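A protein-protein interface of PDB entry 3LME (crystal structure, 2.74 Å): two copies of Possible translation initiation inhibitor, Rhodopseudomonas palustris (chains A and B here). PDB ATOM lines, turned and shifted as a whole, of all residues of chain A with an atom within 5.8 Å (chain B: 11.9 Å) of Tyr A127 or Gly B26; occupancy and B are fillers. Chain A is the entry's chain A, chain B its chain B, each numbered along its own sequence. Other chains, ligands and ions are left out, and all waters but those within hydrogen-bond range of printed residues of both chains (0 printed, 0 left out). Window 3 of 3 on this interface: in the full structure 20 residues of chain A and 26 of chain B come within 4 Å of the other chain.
OH of Tyr A127 lies close to N of Gly B26 (3.2 Å).
No residue of chain B comes within 4 Å of Asp A27. Phe A28 touches just these residues of chain B: Ala B25, Phe B28 and Phe B30. No residue of chain B comes within 4 Å of Val A29. Of chain B, only Leu B3 (3.5 Å) comes within 4 Å of Ala A73. No residue of chain B comes within 4 Å of Thr A125. No residue of chain B comes within 4 Å of Phe A126. Of chain B, only Ser B2 (3.6 Å), Leu B3 (3.7 Å), Ala B25 (3.3 Å) and Gly B26 (3.2 Å) come within 4 Å of Tyr A127. No residue of chain B comes within 4 Å of Ala A128. No residue of chain B comes within 4 Å of Pro A129. Printed residues of chain A within 4 Å of Ser B2: Tyr A127. Of the printed residues of chain A, Leu B3 touches Asp A72 (3.4 Å), Ala A73 (3.5 Å), Val A74 (3.7 Å) and Tyr A127 (3.7 Å). Of the printed residues of chain A, Ala B25 touches Phe A28 (3.8 Å), Val A74 (3.7 Å) and Tyr A127 (3.3 Å). Gly B26 touches just one residue of chain A: Tyr A127. Of the printed residues of chain A, Phe B30 touches Phe A28 and Val A74.
Among the printed residues, merely in contact across the chains: Tyr A127 with Ala B25, Asp A72 with Leu B3, Ala A73 with Leu B3, Val A74 with Phe B30, Tyr A127 with Ser B2, Phe A28 with Phe B30, Val A74 with Ala B25, Tyr A127 with Leu B3, Val A74 with Leu B3, Phe A28 with Ala B25 and Phe A28 with Phe B28.
The backbone carbonyl oxygen (O) of Thr A125 lies within hydrogen-bond range of the backbone NH (N) of Val A74 (2.8 Å). The backbone NH (N) of Tyr A127 lies within hydrogen-bond range of the backbone carbonyl oxygen (O) of Asp A72. The backbone carbonyl oxygen of Ala B23 sits at hydrogen-bond distance from the backbone NH of Phe B30 (2.7 Å). The guanidinium group of Arg B24 lies within hydrogen-bond range of the backbone carbonyl oxygen of Gly B26 (3.3 Å).
Phe B28 touches its own counterpart, Phe A28. Of the 12 pairs that touch across the chains among the printed residues, 1 has its exchanged pair printed and touching as well.
Of the 27 printed residues of chain B, 6 touch a printed residue of chain A. Of the 13 printed residues of chain A, 5 touch a printed residue of chain B. Hydrophobic or aromatic side chains of chain A that line the printed part of chain B: Phe A28, Val A74 and Tyr A127. Among the printed residues, no Asp or Glu carboxylate lies within 4 Å of a Lys or Arg side-chain nitrogen of the other chain.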
ATOM      1  N   ARG A  24       4.513 -16.400  35.624  1.00  0.00           N
ATOM      2  CA  ARG A  24       4.372 -17.482  34.673  1.00  0.00           C
ATOM      3  C   ARG A  24       2.898 -17.620  34.341  1.00  0.00           C
ATOM      4  O   ARG A  24       2.053 -17.668  35.238  1.00  0.00           O
ATOM      5  CB  ARG A  24       4.865 -18.781  35.285  1.00  0.00           C
ATOM      6  CG  ARG A  24       4.628 -19.986  34.402  1.00  0.00           C
ATOM      7  CD  ARG A  24       5.877 -20.843  34.302  1.00  0.00           C
ATOM      8  NE  ARG A  24       5.990 -21.304  32.930  1.00  0.00           N
ATOM      9  CZ  ARG A  24       7.127 -21.463  32.268  1.00  0.00           C
ATOM     10  NH1 ARG A  24       8.295 -21.205  32.842  1.00  0.00           N
ATOM     11  NH2 ARG A  24       7.081 -21.876  31.012  1.00  0.00           N
ATOM     12  N   ASP A  27       2.727 -21.348  29.266  1.00  0.00           N
ATOM     13  CA  ASP A  27       4.060 -21.422  28.654  1.00  0.00           C
ATOM     14  C   ASP A  27       4.784 -20.094  28.671  1.00  0.00           C
ATOM     15  O   ASP A  27       6.010 -20.067  28.467  1.00  0.00           O
ATOM     16  CB  ASP A  27       3.999 -21.897  27.199  1.00  0.00           C
ATOM     17  CG  ASP A  27       3.423 -23.281  27.063  1.00  0.00           C
ATOM     18  OD1 ASP A  27       3.546 -24.103  28.019  1.00  0.00           O
ATOM     19  OD2 ASP A  27       2.822 -23.536  25.991  1.00  0.00           O
ATOM     20  N   PHE A  28       4.047 -19.001  28.884  1.00  0.00           N
ATOM     21  CA  PHE A  28       4.655 -17.693  28.796  1.00  0.00           C
ATOM     22  C   PHE A  28       5.136 -17.156  30.129  1.00  0.00           C
ATOM     23  O   PHE A  28       4.582 -17.506  31.184  1.00  0.00           O
ATOM     24  CB  PHE A  28       3.709 -16.709  28.158  1.00  0.00           C
ATOM     25  CG  PHE A  28       3.518 -16.929  26.711  1.00  0.00           C
ATOM     26  CD1 PHE A  28       4.247 -16.195  25.789  1.00  0.00           C
ATOM     27  CD2 PHE A  28       2.601 -17.877  26.253  1.00  0.00           C
ATOM     28  CE1 PHE A  28       4.063 -16.402  24.429  1.00  0.00           C
ATOM     29  CE2 PHE A  28       2.404 -18.089  24.907  1.00  0.00           C
ATOM     30  CZ  PHE A  28       3.137 -17.359  23.992  1.00  0.00           C
ATOM     31  N   VAL A  29       6.165 -16.307  30.077  1.00  0.00           N
ATOM     32  CA  VAL A  29       6.677 -15.623  31.254  1.00  0.00           C
ATOM     33  C   VAL A  29       6.801 -14.117  31.016  1.00  0.00           C
ATOM     34  O   VAL A  29       7.529 -13.671  30.105  1.00  0.00           O
ATOM     35  CB  VAL A  29       8.021 -16.180  31.637  1.00  0.00           C
ATOM     36  CG1 VAL A  29       8.647 -15.342  32.750  1.00  0.00           C
ATOM     37  CG2 VAL A  29       7.863 -17.650  32.045  1.00  0.00           C
ATOM     38  N   ALA A  68      12.788 -19.521  32.204  1.00  0.00           N
ATOM     39  CA  ALA A  68      13.061 -19.020  30.874  1.00  0.00           C
ATOM     40  C   ALA A  68      14.486 -18.578  30.802  1.00  0.00           C
ATOM     41  O   ALA A  68      15.046 -18.109  31.787  1.00  0.00           O
ATOM     42  CB  ALA A  68      12.167 -17.876  30.559  1.00  0.00           C
ATOM     43  N   ASP A  72      14.696 -17.598  25.050  1.00  0.00           N
ATOM     44  CA  ASP A  72      13.247 -17.675  25.073  1.00  0.00           C
ATOM     45  C   ASP A  72      12.568 -16.320  24.932  1.00  0.00           C
ATOM     46  O   ASP A  72      11.349 -16.266  25.080  1.00  0.00           O
ATOM     47  CB  ASP A  72      12.775 -18.332  26.384  1.00  0.00           C
ATOM     48  CG  ASP A  72      13.340 -19.744  26.572  1.00  0.00           C
ATOM     49  OD1 ASP A  72      13.706 -20.347  25.555  1.00  0.00           O
ATOM     50  OD2 ASP A  72      13.423 -20.255  27.718  1.00  0.00           O
ATOM     51  N   ALA A  73      13.306 -15.233  24.669  1.00  0.00           N
ATOM     52  CA  ALA A  73      12.680 -13.894  24.626  1.00  0.00           C
ATOM     53  C   ALA A  73      11.840 -13.700  23.376  1.00  0.00           C
ATOM     54  O   ALA A  73      12.348 -13.846  22.289  1.00  0.00           O
ATOM     55  CB  ALA A  73      13.700 -12.820  24.708  1.00  0.00           C
ATOM     56  N   VAL A  74      10.552 -13.400  23.512  1.00  0.00           N
ATOM     57  CA  VAL A  74       9.731 -13.097  22.325  1.00  0.00           C
ATOM     58  C   VAL A  74       9.503 -11.612  22.131  1.00  0.00           C
ATOM     59  O   VAL A  74       9.149 -11.207  21.038  1.00  0.00           O
ATOM     60  CB  VAL A  74       8.386 -13.830  22.277  1.00  0.00           C
ATOM     61  CG1 VAL A  74       8.601 -15.338  22.247  1.00  0.00           C
ATOM     62  CG2 VAL A  74       7.543 -13.462  23.452  1.00  0.00           C
ATOM     63  N   THR A 125       9.245 -10.367  27.698  1.00  0.00           N
ATOM     64  CA  THR A 125       8.239 -11.435  27.601  1.00  0.00           C
ATOM     65  C   THR A 125       8.892 -12.676  26.983  1.00  0.00           C
ATOM     66  O   THR A 125       9.566 -12.590  25.965  1.00  0.00           O
ATOM     67  CB  THR A 125       7.056 -10.965  26.751  1.00  0.00           C
ATOM     68  OG1 THR A 125       6.616  -9.709  27.260  1.00  0.00           O
ATOM     69  CG2 THR A 125       5.903 -11.959  26.784  1.00  0.00           C
ATOM     70  N   PHE A 126       8.719 -13.818  27.634  1.00  0.00           N
ATOM     71  CA  PHE A 126       9.436 -15.029  27.251  1.00  0.00           C
ATOM     72  C   PHE A 126       8.460 -16.181  26.991  1.00  0.00           C
ATOM     73  O   PHE A 126       7.373 -16.252  27.590  1.00  0.00           O
ATOM     74  CB  PHE A 126      10.427 -15.432  28.339  1.00  0.00           C
ATOM     75  CG  PHE A 126      11.502 -14.400  28.624  1.00  0.00           C
ATOM     76  CD1 PHE A 126      11.211 -13.225  29.323  1.00  0.00           C
ATOM     77  CD2 PHE A 126      12.807 -14.629  28.249  1.00  0.00           C
ATOM     78  CE1 PHE A 126      12.200 -12.294  29.590  1.00  0.00           C
ATOM     79  CE2 PHE A 126      13.802 -13.706  28.516  1.00  0.00           C
ATOM     80  CZ  PHE A 126      13.507 -12.533  29.181  1.00  0.00           C
ATOM     81  N   TYR A 127       8.857 -17.080  26.090  1.00  0.00           N
ATOM     82  CA  TYR A 127       8.109 -18.294  25.793  1.00  0.00           C
ATOM     83  C   TYR A 127       8.978 -19.423  26.209  1.00  0.00           C
ATOM     84  O   TYR A 127      10.018 -19.630  25.578  1.00  0.00           O
ATOM     85  CB  TYR A 127       7.916 -18.422  24.302  1.00  0.00           C
ATOM     86  CG  TYR A 127       7.163 -19.645  23.857  1.00  0.00           C
ATOM     87  CD1 TYR A 127       5.885 -19.920  24.348  1.00  0.00           C
ATOM     88  CD2 TYR A 127       7.698 -20.495  22.896  1.00  0.00           C
ATOM     89  CE1 TYR A 127       5.161 -21.033  23.914  1.00  0.00           C
ATOM     90  CE2 TYR A 127       6.997 -21.600  22.445  1.00  0.00           C
ATOM     91  CZ  TYR A 127       5.722 -21.872  22.965  1.00  0.00           C
ATOM     92  OH  TYR A 127       5.024 -22.980  22.527  1.00  0.00           O
ATOM     93  N   ALA A 128       8.564 -20.163  27.236  1.00  0.00           N
ATOM     94  CA  ALA A 128       9.383 -21.230  27.769  1.00  0.00           C
ATOM     95  C   ALA A 128       8.560 -22.465  28.129  1.00  0.00           C
ATOM     96  O   ALA A 128       8.362 -22.739  29.316  1.00  0.00           O
ATOM     97  CB  ALA A 128      10.110 -20.722  28.985  1.00  0.00           C
ATOM     98  N   PRO A 129       8.089 -23.237  27.121  1.00  0.00           N
ATOM     99  CA  PRO A 129       7.181 -24.368  27.395  1.00  0.00           C
ATOM    100  C   PRO A 129       7.713 -25.297  28.476  1.00  0.00           C
ATOM    101  O   PRO A 129       8.919 -25.489  28.570  1.00  0.00           O
ATOM    102  CB  PRO A 129       7.151 -25.114  26.067  1.00  0.00           C
ATOM    103  CG  PRO A 129       7.410 -24.110  25.070  1.00  0.00           C
ATOM    104  CD  PRO A 129       8.403 -23.141  25.685  1.00  0.00           C
ATOM    105  N   SER B   2       9.838 -25.217  20.735  1.00  0.00           N
ATOM    106  CA  SER B   2       9.787 -23.909  21.421  1.00  0.00           C
ATOM    107  C   SER B   2       9.727 -22.729  20.423  1.00  0.00           C
ATOM    108  O   SER B   2       8.982 -22.774  19.440  1.00  0.00           O
ATOM    109  CB  SER B   2      10.939 -23.783  22.427  1.00  0.00           C
ATOM    110  OG  SER B   2      12.178 -23.710  21.761  1.00  0.00           O
ATOM    111  N   LEU B   3      10.456 -21.662  20.689  1.00  0.00           N
ATOM    112  CA  LEU B   3      10.264 -20.408  19.961  1.00  0.00           C
ATOM    113  C   LEU B   3      10.878 -20.470  18.552  1.00  0.00           C
ATOM    114  O   LEU B   3      11.867 -21.147  18.333  1.00  0.00           O
ATOM    115  CB  LEU B   3      10.813 -19.266  20.842  1.00  0.00           C
ATOM    116  CG  LEU B   3      11.488 -17.931  20.484  1.00  0.00           C
ATOM    117  CD1 LEU B   3      11.783 -17.212  21.746  1.00  0.00           C
ATOM    118  CD2 LEU B   3      12.795 -18.054  19.709  1.00  0.00           C
ATOM    119  N   LYS B   4      10.302 -19.750  17.602  1.00  0.00           N
ATOM    120  CA  LYS B   4      10.767 -19.772  16.212  1.00  0.00           C
ATOM    121  C   LYS B   4      10.947 -18.339  15.646  1.00  0.00           C
ATOM    122  O   LYS B   4       9.963 -17.667  15.332  1.00  0.00           O
ATOM    123  CB  LYS B   4       9.753 -20.559  15.374  1.00  0.00           C
ATOM    124  CG  LYS B   4      10.343 -21.536  14.333  1.00  0.00           C
ATOM    125  CD  LYS B   4      10.863 -20.837  13.043  1.00  0.00           C
ATOM    126  CE  LYS B   4      11.243 -21.877  11.941  1.00  0.00           C
ATOM    127  NZ  LYS B   4      10.071 -22.353  11.101  1.00  0.00           N
ATOM    128  N   ILE B   5      12.184 -17.866  15.530  1.00  0.00           N
ATOM    129  CA  ILE B   5      12.456 -16.534  14.978  1.00  0.00           C
ATOM    130  C   ILE B   5      11.927 -16.448  13.545  1.00  0.00           C
ATOM    131  O   ILE B   5      12.119 -17.376  12.767  1.00  0.00           O
ATOM    132  CB  ILE B   5      13.969 -16.215  15.000  1.00  0.00           C
ATOM    133  CG1 ILE B   5      14.484 -16.018  16.438  1.00  0.00           C
ATOM    134  CG2 ILE B   5      14.312 -15.028  14.111  1.00  0.00           C
ATOM    135  CD1 ILE B   5      13.738 -14.998  17.310  1.00  0.00           C
ATOM    136  N   ILE B   6      11.239 -15.370  13.192  1.00  0.00           N
ATOM    137  CA  ILE B   6      10.750 -15.258  11.835  1.00  0.00           C
ATOM    138  C   ILE B   6      11.879 -14.828  10.908  1.00  0.00           C
ATOM    139  O   ILE B   6      12.467 -13.764  11.094  1.00  0.00           O
ATOM    140  CB  ILE B   6       9.568 -14.289  11.710  1.00  0.00           C
ATOM    141  CG1 ILE B   6       8.447 -14.706  12.664  1.00  0.00           C
ATOM    142  CG2 ILE B   6       9.066 -14.252  10.261  1.00  0.00           C
ATOM    143  CD1 ILE B   6       7.361 -13.639  12.869  1.00  0.00           C
ATOM    144  N   GLY B  22      10.676 -10.638  14.045  1.00  0.00           N
ATOM    145  CA  GLY B  22       9.713 -11.094  15.018  1.00  0.00           C
ATOM    146  C   GLY B  22       9.832 -12.552  15.332  1.00  0.00           C
ATOM    147  O   GLY B  22      10.703 -13.232  14.803  1.00  0.00           O
ATOM    148  N   ALA B  23       8.953 -13.024  16.200  1.00  0.00           N
ATOM    149  CA  ALA B  23       8.947 -14.426  16.580  1.00  0.00           C
ATOM    150  C   ALA B  23       7.575 -15.085  16.701  1.00  0.00           C
ATOM    151  O   ALA B  23       6.572 -14.464  17.075  1.00  0.00           O
ATOM    152  CB  ALA B  23       9.696 -14.613  17.857  1.00  0.00           C
ATOM    153  N   ARG B  24       7.553 -16.371  16.406  1.00  0.00           N
ATOM    154  CA  ARG B  24       6.391 -17.174  16.682  1.00  0.00           C
ATOM    155  C   ARG B  24       6.626 -18.002  17.931  1.00  0.00           C
ATOM    156  O   ARG B  24       7.657 -18.649  18.042  1.00  0.00           O
ATOM    157  CB  ARG B  24       6.153 -18.104  15.513  1.00  0.00           C
ATOM    158  CG  ARG B  24       5.310 -19.300  15.874  1.00  0.00           C
ATOM    159  CD  ARG B  24       4.464 -19.716  14.714  1.00  0.00           C
ATOM    160  NE  ARG B  24       3.131 -19.933  15.219  1.00  0.00           N
ATOM    161  CZ  ARG B  24       2.028 -19.536  14.613  1.00  0.00           C
ATOM    162  NH1 ARG B  24       2.066 -18.900  13.452  1.00  0.00           N
ATOM    163  NH2 ARG B  24       0.874 -19.786  15.194  1.00  0.00           N
ATOM    164  N   ALA B  25       5.679 -17.992  18.859  1.00  0.00           N
ATOM    165  CA  ALA B  25       5.790 -18.791  20.071  1.00  0.00           C
ATOM    166  C   ALA B  25       4.456 -19.469  20.292  1.00  0.00           C
ATOM    167  O   ALA B  25       3.433 -18.796  20.494  1.00  0.00           O
ATOM    168  CB  ALA B  25       6.149 -17.904  21.257  1.00  0.00           C
ATOM    169  N   GLY B  26       4.441 -20.800  20.209  1.00  0.00           N
ATOM    170  CA  GLY B  26       3.193 -21.565  20.318  1.00  0.00           C
ATOM    171  C   GLY B  26       2.161 -21.039  19.359  1.00  0.00           C
ATOM    172  O   GLY B  26       2.354 -21.069  18.165  1.00  0.00           O
ATOM    173  N   ASP B  27       1.083 -20.490  19.881  1.00  0.00           N
ATOM    174  CA  ASP B  27      -0.004 -20.033  19.021  1.00  0.00           C
ATOM    175  C   ASP B  27       0.068 -18.560  18.654  1.00  0.00           C
ATOM    176  O   ASP B  27      -0.847 -18.047  18.020  1.00  0.00           O
ATOM    177  CB  ASP B  27      -1.342 -20.326  19.690  1.00  0.00           C
ATOM    178  CG  ASP B  27      -1.697 -21.811  19.672  1.00  0.00           C
ATOM    179  OD1 ASP B  27      -1.202 -22.561  18.782  1.00  0.00           O
ATOM    180  OD2 ASP B  27      -2.482 -22.230  20.555  1.00  0.00           O
ATOM    181  N   PHE B  28       1.143 -17.881  19.055  1.00  0.00           N
ATOM    182  CA  PHE B  28       1.181 -16.418  19.013  1.00  0.00           C
ATOM    183  C   PHE B  28       2.325 -15.961  18.174  1.00  0.00           C
ATOM    184  O   PHE B  28       3.318 -16.661  18.074  1.00  0.00           O
ATOM    185  CB  PHE B  28       1.377 -15.826  20.416  1.00  0.00           C
ATOM    186  CG  PHE B  28       0.156 -15.847  21.265  1.00  0.00           C
ATOM    187  CD1 PHE B  28      -0.680 -14.714  21.332  1.00  0.00           C
ATOM    188  CD2 PHE B  28      -0.164 -16.983  22.019  1.00  0.00           C
ATOM    189  CE1 PHE B  28      -1.858 -14.715  22.137  1.00  0.00           C
ATOM    190  CE2 PHE B  28      -1.310 -17.002  22.840  1.00  0.00           C
ATOM    191  CZ  PHE B  28      -2.169 -15.855  22.902  1.00  0.00           C
ATOM    192  N   VAL B  29       2.208 -14.770  17.607  1.00  0.00           N
ATOM    193  CA  VAL B  29       3.275 -14.211  16.814  1.00  0.00           C
ATOM    194  C   VAL B  29       3.549 -12.801  17.320  1.00  0.00           C
ATOM    195  O   VAL B  29       2.620 -11.998  17.420  1.00  0.00           O
ATOM    196  CB  VAL B  29       2.888 -14.177  15.338  1.00  0.00           C
ATOM    197  CG1 VAL B  29       3.928 -13.411  14.526  1.00  0.00           C
ATOM    198  CG2 VAL B  29       2.741 -15.583  14.820  1.00  0.00           C
ATOM    199  N   PHE B  30       4.807 -12.515  17.665  1.00  0.00           N
ATOM    200  CA  PHE B  30       5.191 -11.191  18.159  1.00  0.00           C
ATOM    201  C   PHE B  30       6.076 -10.498  17.159  1.00  0.00           C
ATOM    202  O   PHE B  30       7.119 -11.024  16.825  1.00  0.00           O
ATOM    203  CB  PHE B  30       5.971 -11.298  19.465  1.00  0.00           C
ATOM    204  CG  PHE B  30       5.229 -11.954  20.571  1.00  0.00           C
ATOM    205  CD1 PHE B  30       4.656 -11.190  21.581  1.00  0.00           C
ATOM    206  CD2 PHE B  30       5.139 -13.331  20.643  1.00  0.00           C
ATOM    207  CE1 PHE B  30       3.980 -11.801  22.660  1.00  0.00           C
ATOM    208  CE2 PHE B  30       4.452 -13.957  21.710  1.00  0.00           C
ATOM    209  CZ  PHE B  30       3.879 -13.189  22.724  1.00  0.00           C
ATOM    210  N   ALA B  63       4.177 -10.398   9.999  1.00  0.00           N
ATOM    211  CA  ALA B  63       3.193 -11.288  10.587  1.00  0.00           C
ATOM    212  C   ALA B  63       2.760 -12.410   9.630  1.00  0.00           C
ATOM    213  O   ALA B  63       2.562 -13.529  10.064  1.00  0.00           O
ATOM    214  CB  ALA B  63       1.981 -10.488  11.138  1.00  0.00           C
ATOM    215  N   ALA B  65       4.634 -13.765   7.166  1.00  0.00           N
ATOM    216  CA  ALA B  65       5.772 -14.650   7.090  1.00  0.00           C
ATOM    217  C   ALA B  65       5.701 -15.697   8.186  1.00  0.00           C
ATOM    218  O   ALA B  65       6.472 -16.668   8.173  1.00  0.00           O
ATOM    219  CB  ALA B  65       7.039 -13.852   7.223  1.00  0.00           C
ATOM    220  N   ALA B  66       4.804 -15.476   9.154  1.00  0.00           N
ATOM    221  CA  ALA B  66       4.674 -16.375  10.288  1.00  0.00           C
ATOM    222  C   ALA B  66       3.283 -16.967  10.403  1.00  0.00           C
ATOM    223  O   ALA B  66       2.977 -17.642  11.378  1.00  0.00           O
ATOM    224  CB  ALA B  66       5.063 -15.690  11.554  1.00  0.00           C
ATOM    225  N   GLY B  67       2.440 -16.733   9.410  1.00  0.00           N
ATOM    226  CA  GLY B  67       1.145 -17.389   9.387  1.00  0.00           C
ATOM    227  C   GLY B  67       0.011 -16.614  10.035  1.00  0.00           C
ATOM    228  O   GLY B  67      -1.030 -17.189  10.365  1.00  0.00           O
ATOM    229  N   ALA B  68       0.199 -15.306  10.185  1.00  0.00           N
ATOM    230  CA  ALA B  68      -0.790 -14.454  10.827  1.00  0.00           C
ATOM    231  C   ALA B  68      -1.243 -13.314   9.922  1.00  0.00           C
ATOM    232  O   ALA B  68      -0.459 -12.708   9.152  1.00  0.00           O
ATOM    233  CB  ALA B  68      -0.268 -13.926  12.131  1.00  0.00           C
ATOM    234  N   ASP B  72      -5.794 -11.462  12.872  1.00  0.00           N
ATOM    235  CA  ASP B  72      -5.194 -12.135  14.016  1.00  0.00           C
ATOM    236  C   ASP B  72      -4.618 -11.194  15.066  1.00  0.00           C
ATOM    237  O   ASP B  72      -4.125 -11.649  16.081  1.00  0.00           O
ATOM    238  CB  ASP B  72      -4.154 -13.149  13.549  1.00  0.00           C
ATOM    239  CG  ASP B  72      -4.778 -14.244  12.701  1.00  0.00           C
ATOM    240  OD1 ASP B  72      -5.981 -14.457  12.864  1.00  0.00           O
ATOM    241  OD2 ASP B  72      -4.089 -14.894  11.883  1.00  0.00           O
ATOM    242  N   VAL B  74      -4.041  -9.246  18.142  1.00  0.00           N
ATOM    243  CA  VAL B  74      -4.564  -9.103  19.501  1.00  0.00           C
ATOM    244  C   VAL B  74      -4.099  -7.836  20.222  1.00  0.00           C
ATOM    245  O   VAL B  74      -4.685  -7.478  21.230  1.00  0.00           O
ATOM    246  CB  VAL B  74      -4.326 -10.332  20.390  1.00  0.00           C
ATOM    247  CG1 VAL B  74      -5.178 -11.505  19.918  1.00  0.00           C
ATOM    248  CG2 VAL B  74      -2.821 -10.683  20.503  1.00  0.00           C
ATOM    249  N   THR B 125       1.137  -7.628  18.282  1.00  0.00           N
ATOM    250  CA  THR B 125       1.086  -8.985  18.787  1.00  0.00           C
ATOM    251  C   THR B 125      -0.106  -9.704  18.141  1.00  0.00           C
ATOM    252  O   THR B 125      -1.192  -9.124  17.955  1.00  0.00           O
ATOM    253  CB  THR B 125       1.003  -9.000  20.331  1.00  0.00           C
ATOM    254  OG1 THR B 125       2.128  -8.280  20.877  1.00  0.00           O
ATOM    255  CG2 THR B 125       0.999 -10.426  20.878  1.00  0.00           C
ATOM    256  N   PHE B 126       0.117 -10.969  17.787  1.00  0.00           N
ATOM    257  CA  PHE B 126      -0.827 -11.745  16.979  1.00  0.00           C
ATOM    258  C   PHE B 126      -1.098 -13.117  17.561  1.00  0.00           C
ATOM    259  O   PHE B 126      -0.232 -13.690  18.234  1.00  0.00           O
ATOM    260  CB  PHE B 126      -0.290 -11.907  15.563  1.00  0.00           C
ATOM    261  CG  PHE B 126      -0.252 -10.644  14.808  1.00  0.00           C
ATOM    262  CD1 PHE B 126       0.749  -9.721  15.027  1.00  0.00           C
ATOM    263  CD2 PHE B 126      -1.219 -10.360  13.879  1.00  0.00           C
ATOM    264  CE1 PHE B 126       0.768  -8.530  14.319  1.00  0.00           C
ATOM    265  CE2 PHE B 126      -1.201  -9.163  13.160  1.00  0.00           C
ATOM    266  CZ  PHE B 126      -0.214  -8.261  13.378  1.00  0.00           C
ATOM    267  N   TYR B 127      -2.299 -13.623  17.267  1.00  0.00           N
ATOM    268  CA  TYR B 127      -2.765 -14.938  17.690  1.00  0.00           C
ATOM    269  C   TYR B 127      -3.266 -15.679  16.476  1.00  0.00           C
ATOM    270  O   TYR B 127      -4.233 -15.268  15.836  1.00  0.00           O
ATOM    271  CB  TYR B 127      -3.937 -14.794  18.643  1.00  0.00           C
ATOM    272  CG  TYR B 127      -4.471 -16.114  19.149  1.00  0.00           C
ATOM    273  CD1 TYR B 127      -3.656 -16.991  19.847  1.00  0.00           C
ATOM    274  CD2 TYR B 127      -5.793 -16.477  18.945  1.00  0.00           C
ATOM    275  CE1 TYR B 127      -4.138 -18.184  20.314  1.00  0.00           C
ATOM    276  CE2 TYR B 127      -6.278 -17.680  19.408  1.00  0.00           C
ATOM    277  CZ  TYR B 127      -5.444 -18.519  20.094  1.00  0.00           C
ATOM    278  OH  TYR B 127      -5.916 -19.710  20.584  1.00  0.00           O
ATOM    279  N   ALA B 128      -2.624 -16.792  16.172  1.00  0.00           N
ATOM    280  CA  ALA B 128      -2.850 -17.470  14.926  1.00  0.00           C
ATOM    281  C   ALA B 128      -2.569 -18.957  15.094  1.00  0.00           C
ATOM    282  O   ALA B 128      -1.598 -19.465  14.559  1.00  0.00           O
ATOM    283  CB  ALA B 128      -1.968 -16.862  13.853  1.00  0.00           C
ATOM    284  N   PRO B 129      -3.439 -19.670  15.823  1.00  0.00           N
ATOM    285  CA  PRO B 129      -3.176 -21.094  15.994  1.00  0.00           C
ATOM    286  C   PRO B 129      -3.135 -21.779  14.630  1.00  0.00           C
ATOM    287  O   PRO B 129      -3.942 -21.445  13.733  1.00  0.00           O
ATOM    288  CB  PRO B 129      -4.382 -21.597  16.798  1.00  0.00           C
ATOM    289  CG  PRO B 129      -5.188 -20.405  17.160  1.00  0.00           C
ATOM    290  CD  PRO B 129      -4.799 -19.291  16.255  1.00  0.00           C
ATOM    291  N   ALA B 130      -2.176 -22.701  14.477  1.00  0.00           N
ATOM    292  CA  ALA B 130      -2.006 -23.504  13.239  1.00  0.00           C
ATOM    293  C   ALA B 130      -2.909 -24.760  13.243  1.00  0.00           C
ATOM    294  O   ALA B 130      -3.761 -24.933  14.134  1.00  0.00           O
ATOM    295  CB  ALA B 130      -0.485 -23.885  13.002  1.00  0.00           C
